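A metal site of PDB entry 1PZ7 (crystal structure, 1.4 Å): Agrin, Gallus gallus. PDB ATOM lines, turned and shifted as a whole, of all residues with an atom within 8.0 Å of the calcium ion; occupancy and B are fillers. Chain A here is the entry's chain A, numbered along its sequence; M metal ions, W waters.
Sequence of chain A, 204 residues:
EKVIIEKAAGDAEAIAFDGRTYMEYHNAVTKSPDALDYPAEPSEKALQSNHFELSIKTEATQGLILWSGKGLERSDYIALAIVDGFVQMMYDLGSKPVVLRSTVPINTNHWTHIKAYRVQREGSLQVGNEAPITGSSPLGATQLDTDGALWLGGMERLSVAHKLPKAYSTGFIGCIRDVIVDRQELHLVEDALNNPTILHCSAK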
ATOM      1  N   GLU A  44      22.992  11.212 -17.030  1.00  0.00           N
ATOM      2  CA  GLU A  44      23.295  12.539 -17.539  1.00  0.00           C
ATOM      3  C   GLU A  44      22.515  13.627 -16.766  1.00  0.00           C
ATOM      4  O   GLU A  44      21.776  13.319 -15.835  1.00  0.00           O
ATOM      5  CB  GLU A  44      22.920  12.540 -19.034  1.00  0.00           C
ATOM      6  CG  GLU A  44      23.234  13.774 -19.846  1.00  0.00           C
ATOM      7  CD  GLU A  44      22.904  13.587 -21.310  1.00  0.00           C
ATOM      8  OE1 GLU A  44      21.740  13.278 -21.623  1.00  0.00           O
ATOM      9  OE2 GLU A  44      23.810  13.758 -22.155  1.00  0.00           O
ATOM     10  N   LYS A  45      22.721  14.878 -17.154  1.00  0.00           N
ATOM     11  CA  LYS A  45      22.023  16.029 -16.570  1.00  0.00           C
ATOM     12  C   LYS A  45      21.445  16.858 -17.709  1.00  0.00           C
ATOM     13  O   LYS A  45      22.065  16.958 -18.759  1.00  0.00           O
ATOM     14  CB  LYS A  45      23.010  16.897 -15.791  1.00  0.00           C
ATOM     15  CG  LYS A  45      23.701  16.201 -14.635  1.00  0.00           C
ATOM     16  CD  LYS A  45      22.756  15.964 -13.468  1.00  0.00           C
ATOM     17  CE  LYS A  45      22.420  17.252 -12.718  1.00  0.00           C
ATOM     18  NZ  LYS A  45      21.445  18.119 -13.449  1.00  0.00           N
ATOM     19  N   ALA A  46      20.272  17.439 -17.503  1.00  0.00           N
ATOM     20  CA  ALA A  46      19.667  18.314 -18.513  1.00  0.00           C
ATOM     21  C   ALA A  46      19.606  19.725 -17.929  1.00  0.00           C
ATOM     22  O   ALA A  46      18.599  20.128 -17.354  1.00  0.00           O
ATOM     23  CB  ALA A  46      18.277  17.823 -18.875  1.00  0.00           C
ATOM     24  N   LEU A  47      20.696  20.463 -18.074  1.00  0.00           N
ATOM     25  CA  LEU A  47      20.845  21.770 -17.449  1.00  0.00           C
ATOM     26  C   LEU A  47      20.098  22.903 -18.147  1.00  0.00           C
ATOM     27  O   LEU A  47      20.285  23.157 -19.336  1.00  0.00           O
ATOM     28  CB  LEU A  47      22.319  22.152 -17.339  1.00  0.00           C
ATOM     29  CG  LEU A  47      23.187  21.206 -16.509  1.00  0.00           C
ATOM     30  CD1 LEU A  47      24.609  21.726 -16.493  1.00  0.00           C
ATOM     31  CD2 LEU A  47      22.639  21.074 -15.102  1.00  0.00           C
ATOM     32  N   SER A  75      28.119  15.280 -28.353  1.00  0.00           N
ATOM     33  CA  SER A  75      27.738  15.989 -27.137  1.00  0.00           C
ATOM     34  C   SER A  75      27.424  17.471 -27.245  1.00  0.00           C
ATOM     35  O   SER A  75      28.014  18.197 -28.044  1.00  0.00           O
ATOM     36  CB  SER A  75      28.853  15.828 -26.097  1.00  0.00           C
ATOM     37  OG  SER A  75      29.061  14.467 -25.773  1.00  0.00           O
ATOM     38  N   ASP A  76      26.486  17.903 -26.413  1.00  0.00           N
ATOM     39  CA  ASP A  76      26.204  19.309 -26.218  1.00  0.00           C
ATOM     40  C   ASP A  76      27.438  19.906 -25.567  1.00  0.00           C
ATOM     41  O   ASP A  76      28.246  19.184 -24.974  1.00  0.00           O
ATOM     42  CB  ASP A  76      25.050  19.516 -25.239  1.00  0.00           C
ATOM     43  CG  ASP A  76      23.712  19.117 -25.816  1.00  0.00           C
ATOM     44  OD1 ASP A  76      22.728  19.183 -25.042  1.00  0.00           O
ATOM     45  OD2 ASP A  76      23.544  18.752 -26.991  1.00  0.00           O
ATOM     46  N   TYR A  77      27.581  21.213 -25.645  1.00  0.00           N
ATOM     47  CA  TYR A  77      28.695  21.875 -24.992  1.00  0.00           C
ATOM     48  C   TYR A  77      28.433  23.352 -24.840  1.00  0.00           C
ATOM     49  O   TYR A  77      27.607  23.921 -25.537  1.00  0.00           O
ATOM     50  CB  TYR A  77      29.982  21.692 -25.808  1.00  0.00           C
ATOM     51  CG  TYR A  77      29.865  22.234 -27.213  1.00  0.00           C
ATOM     52  CD1 TYR A  77      30.215  23.544 -27.506  1.00  0.00           C
ATOM     53  CD2 TYR A  77      29.376  21.441 -28.240  1.00  0.00           C
ATOM     54  CE1 TYR A  77      30.096  24.056 -28.785  1.00  0.00           C
ATOM     55  CE2 TYR A  77      29.256  21.939 -29.517  1.00  0.00           C
ATOM     56  CZ  TYR A  77      29.609  23.231 -29.779  1.00  0.00           C
ATOM     57  OH  TYR A  77      29.471  23.716 -31.067  1.00  0.00           O
ATOM     58  N   ASP A  92      26.074  24.631 -28.142  1.00  0.00           N
ATOM     59  CA  ASP A  92      25.173  23.875 -28.988  1.00  0.00           C
ATOM     60  C   ASP A  92      24.422  22.977 -28.032  1.00  0.00           C
ATOM     61  O   ASP A  92      25.044  22.189 -27.311  1.00  0.00           O
ATOM     62  CB  ASP A  92      25.950  23.050 -30.027  1.00  0.00           C
ATOM     63  CG  ASP A  92      25.037  22.395 -31.064  1.00  0.00           C
ATOM     64  OD1 ASP A  92      25.542  21.977 -32.130  1.00  0.00           O
ATOM     65  OD2 ASP A  92      23.817  22.263 -30.877  1.00  0.00           O
ATOM     66  N   LEU A  93      23.113  23.131 -27.985  1.00  0.00           N
ATOM     67  CA  LEU A  93      22.239  22.385 -27.072  1.00  0.00           C
ATOM     68  C   LEU A  93      21.493  21.274 -27.807  1.00  0.00           C
ATOM     69  O   LEU A  93      20.685  20.571 -27.202  1.00  0.00           O
ATOM     70  CB  LEU A  93      21.220  23.339 -26.452  1.00  0.00           C
ATOM     71  CG  LEU A  93      21.761  24.619 -25.817  1.00  0.00           C
ATOM     72  CD1 LEU A  93      20.627  25.482 -25.283  1.00  0.00           C
ATOM     73  CD2 LEU A  93      22.735  24.295 -24.704  1.00  0.00           C
ATOM     74  N   GLY A  94      21.782  21.118 -29.093  1.00  0.00           N
ATOM     75  CA  GLY A  94      21.115  20.131 -29.920  1.00  0.00           C
ATOM     76  C   GLY A  94      20.319  20.709 -31.089  1.00  0.00           C
ATOM     77  O   GLY A  94      19.651  19.957 -31.796  1.00  0.00           O
ATOM     78  N   SER A  95      20.396  22.026 -31.265  1.00  0.00           N
ATOM     79  CA  SER A  95      19.703  22.700 -32.367  1.00  0.00           C
ATOM     80  C   SER A  95      20.654  23.637 -33.099  1.00  0.00           C
ATOM     81  O   SER A  95      20.222  24.635 -33.680  1.00  0.00           O
ATOM     82  CB  SER A  95      18.504  23.485 -31.828  1.00  0.00           C
ATOM     83  OG  SER A  95      17.527  22.607 -31.287  1.00  0.00           O
ATOM     84  N   ARG A 118      24.135  31.410 -19.487  1.00  0.00           N
ATOM     85  CA  ARG A 118      23.126  30.943 -20.408  1.00  0.00           C
ATOM     86  C   ARG A 118      21.916  30.523 -19.592  1.00  0.00           C
ATOM     87  O   ARG A 118      22.059  29.857 -18.569  1.00  0.00           O
ATOM     88  CB  ARG A 118      23.646  29.738 -21.196  1.00  0.00           C
ATOM     89  CG  ARG A 118      22.594  29.105 -22.115  1.00  0.00           C
ATOM     90  CD  ARG A 118      22.963  27.725 -22.635  1.00  0.00           C
ATOM     91  NE  ARG A 118      23.020  26.753 -21.554  1.00  0.00           N
ATOM     92  CZ  ARG A 118      21.996  26.019 -21.114  1.00  0.00           C
ATOM     93  NH1 ARG A 118      20.788  26.124 -21.663  1.00  0.00           N
ATOM     94  NH2 ARG A 118      22.185  25.174 -20.114  1.00  0.00           N
ATOM     95  N   GLY A 140      14.388  25.425 -30.467  1.00  0.00           N
ATOM     96  CA  GLY A 140      14.367  23.990 -30.326  1.00  0.00           C
ATOM     97  C   GLY A 140      14.870  23.604 -28.949  1.00  0.00           C
ATOM     98  O   GLY A 140      14.167  23.759 -27.942  1.00  0.00           O
ATOM     99  N   ALA A 141      16.102  23.111 -28.899  1.00  0.00           N
ATOM    100  CA  ALA A 141      16.705  22.673 -27.635  1.00  0.00           C
ATOM    101  C   ALA A 141      17.000  23.842 -26.697  1.00  0.00           C
ATOM    102  O   ALA A 141      17.420  24.913 -27.139  1.00  0.00           O
ATOM    103  CB  ALA A 141      17.977  21.886 -27.925  1.00  0.00           C
ATOM    104  N   THR A 142      16.781  23.625 -25.406  1.00  0.00           N
ATOM    105  CA  THR A 142      16.991  24.648 -24.385  1.00  0.00           C
ATOM    106  C   THR A 142      17.854  24.161 -23.239  1.00  0.00           C
ATOM    107  O   THR A 142      18.215  24.936 -22.364  1.00  0.00           O
ATOM    108  CB  THR A 142      15.651  25.079 -23.764  1.00  0.00           C
ATOM    109  OG1 THR A 142      15.096  24.004 -22.980  1.00  0.00           O
ATOM    110  CG2 THR A 142      14.612  25.366 -24.819  1.00  0.00           C
ATOM    111  N   GLN A 143      18.154  22.868 -23.244  1.00  0.00           N
ATOM    112  CA  GLN A 143      18.888  22.261 -22.146  1.00  0.00           C
ATOM    113  C   GLN A 143      20.229  21.711 -22.615  1.00  0.00           C
ATOM    114  O   GLN A 143      20.353  21.188 -23.711  1.00  0.00           O
ATOM    115  CB  GLN A 143      18.049  21.133 -21.534  1.00  0.00           C
ATOM    116  CG  GLN A 143      16.735  21.645 -20.928  1.00  0.00           C
ATOM    117  CD  GLN A 143      15.638  20.600 -20.911  1.00  0.00           C
ATOM    118  OE1 GLN A 143      15.854  19.441 -21.266  1.00  0.00           O
ATOM    119  NE2 GLN A 143      14.448  21.007 -20.477  1.00  0.00           N
ATOM    120  N   LEU A 144      21.239  21.848 -21.762  1.00  0.00           N
ATOM    121  CA  LEU A 144      22.552  21.322 -22.047  1.00  0.00           C
ATOM    122  C   LEU A 144      22.659  19.969 -21.378  1.00  0.00           C
ATOM    123  O   LEU A 144      22.695  19.867 -20.154  1.00  0.00           O
ATOM    124  CB  LEU A 144      23.639  22.283 -21.555  1.00  0.00           C
ATOM    125  CG  LEU A 144      24.975  22.127 -22.282  1.00  0.00           C
ATOM    126  CD1 LEU A 144      25.826  23.377 -22.123  1.00  0.00           C
ATOM    127  CD2 LEU A 144      25.728  20.889 -21.812  1.00  0.00           C
ATOM    128  N   ASP A 145      22.675  18.923 -22.199  1.00  0.00           N
ATOM    129  CA  ASP A 145      22.750  17.561 -21.697  1.00  0.00           C
ATOM    130  C   ASP A 145      24.209  17.199 -21.475  1.00  0.00           C
ATOM    131  O   ASP A 145      24.996  17.127 -22.424  1.00  0.00           O
ATOM    132  CB  ASP A 145      22.096  16.605 -22.684  1.00  0.00           C
ATOM    133  CG  ASP A 145      20.653  16.961 -22.946  1.00  0.00           C
ATOM    134  OD1 ASP A 145      19.874  16.998 -21.976  1.00  0.00           O
ATOM    135  OD2 ASP A 145      20.225  17.252 -24.082  1.00  0.00           O
ATOM    136  N   THR A 146      24.559  16.966 -20.221  1.00  0.00           N
ATOM    137  CA  THR A 146      25.950  16.726 -19.860  1.00  0.00           C
ATOM    138  C   THR A 146      26.102  15.823 -18.650  1.00  0.00           C
ATOM    139  O   THR A 146      25.172  15.625 -17.877  1.00  0.00           O
ATOM    140  CB  THR A 146      26.658  18.077 -19.575  1.00  0.00           C
ATOM    141  OG1 THR A 146      28.003  17.849 -19.162  1.00  0.00           O
ATOM    142  CG2 THR A 146      26.019  18.789 -18.387  1.00  0.00           C
HETATM  143 CA    CA M   1      20.418  19.413 -25.226  1.00  0.00          CA
HETATM  144  O   HOH W   1      21.094  17.532 -27.163  1.00  0.00           O
HETATM  145  O   HOH W   2      18.045  19.069 -25.363  1.00  0.00           O
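O of Leu 93 is bound to the calcium ion (2.3 Å).
OD1 of Asp 76 is bound to the calcium ion (2.3 Å).
The calcium ion is bound by O of Gln 143 (2.3 Å).
The calcium ion is bound by water W2 (2.4 Å).
OD2 of Asp 145 binds the calcium ion.
Water W1 is bound to the calcium ion, 2.8 Å away.
Of the 19 residues printed, 4 come within 4 Å of the calcium ion.
The nearest printed residue that does not touch the calcium ion is Leu 144 (4.3 Å).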
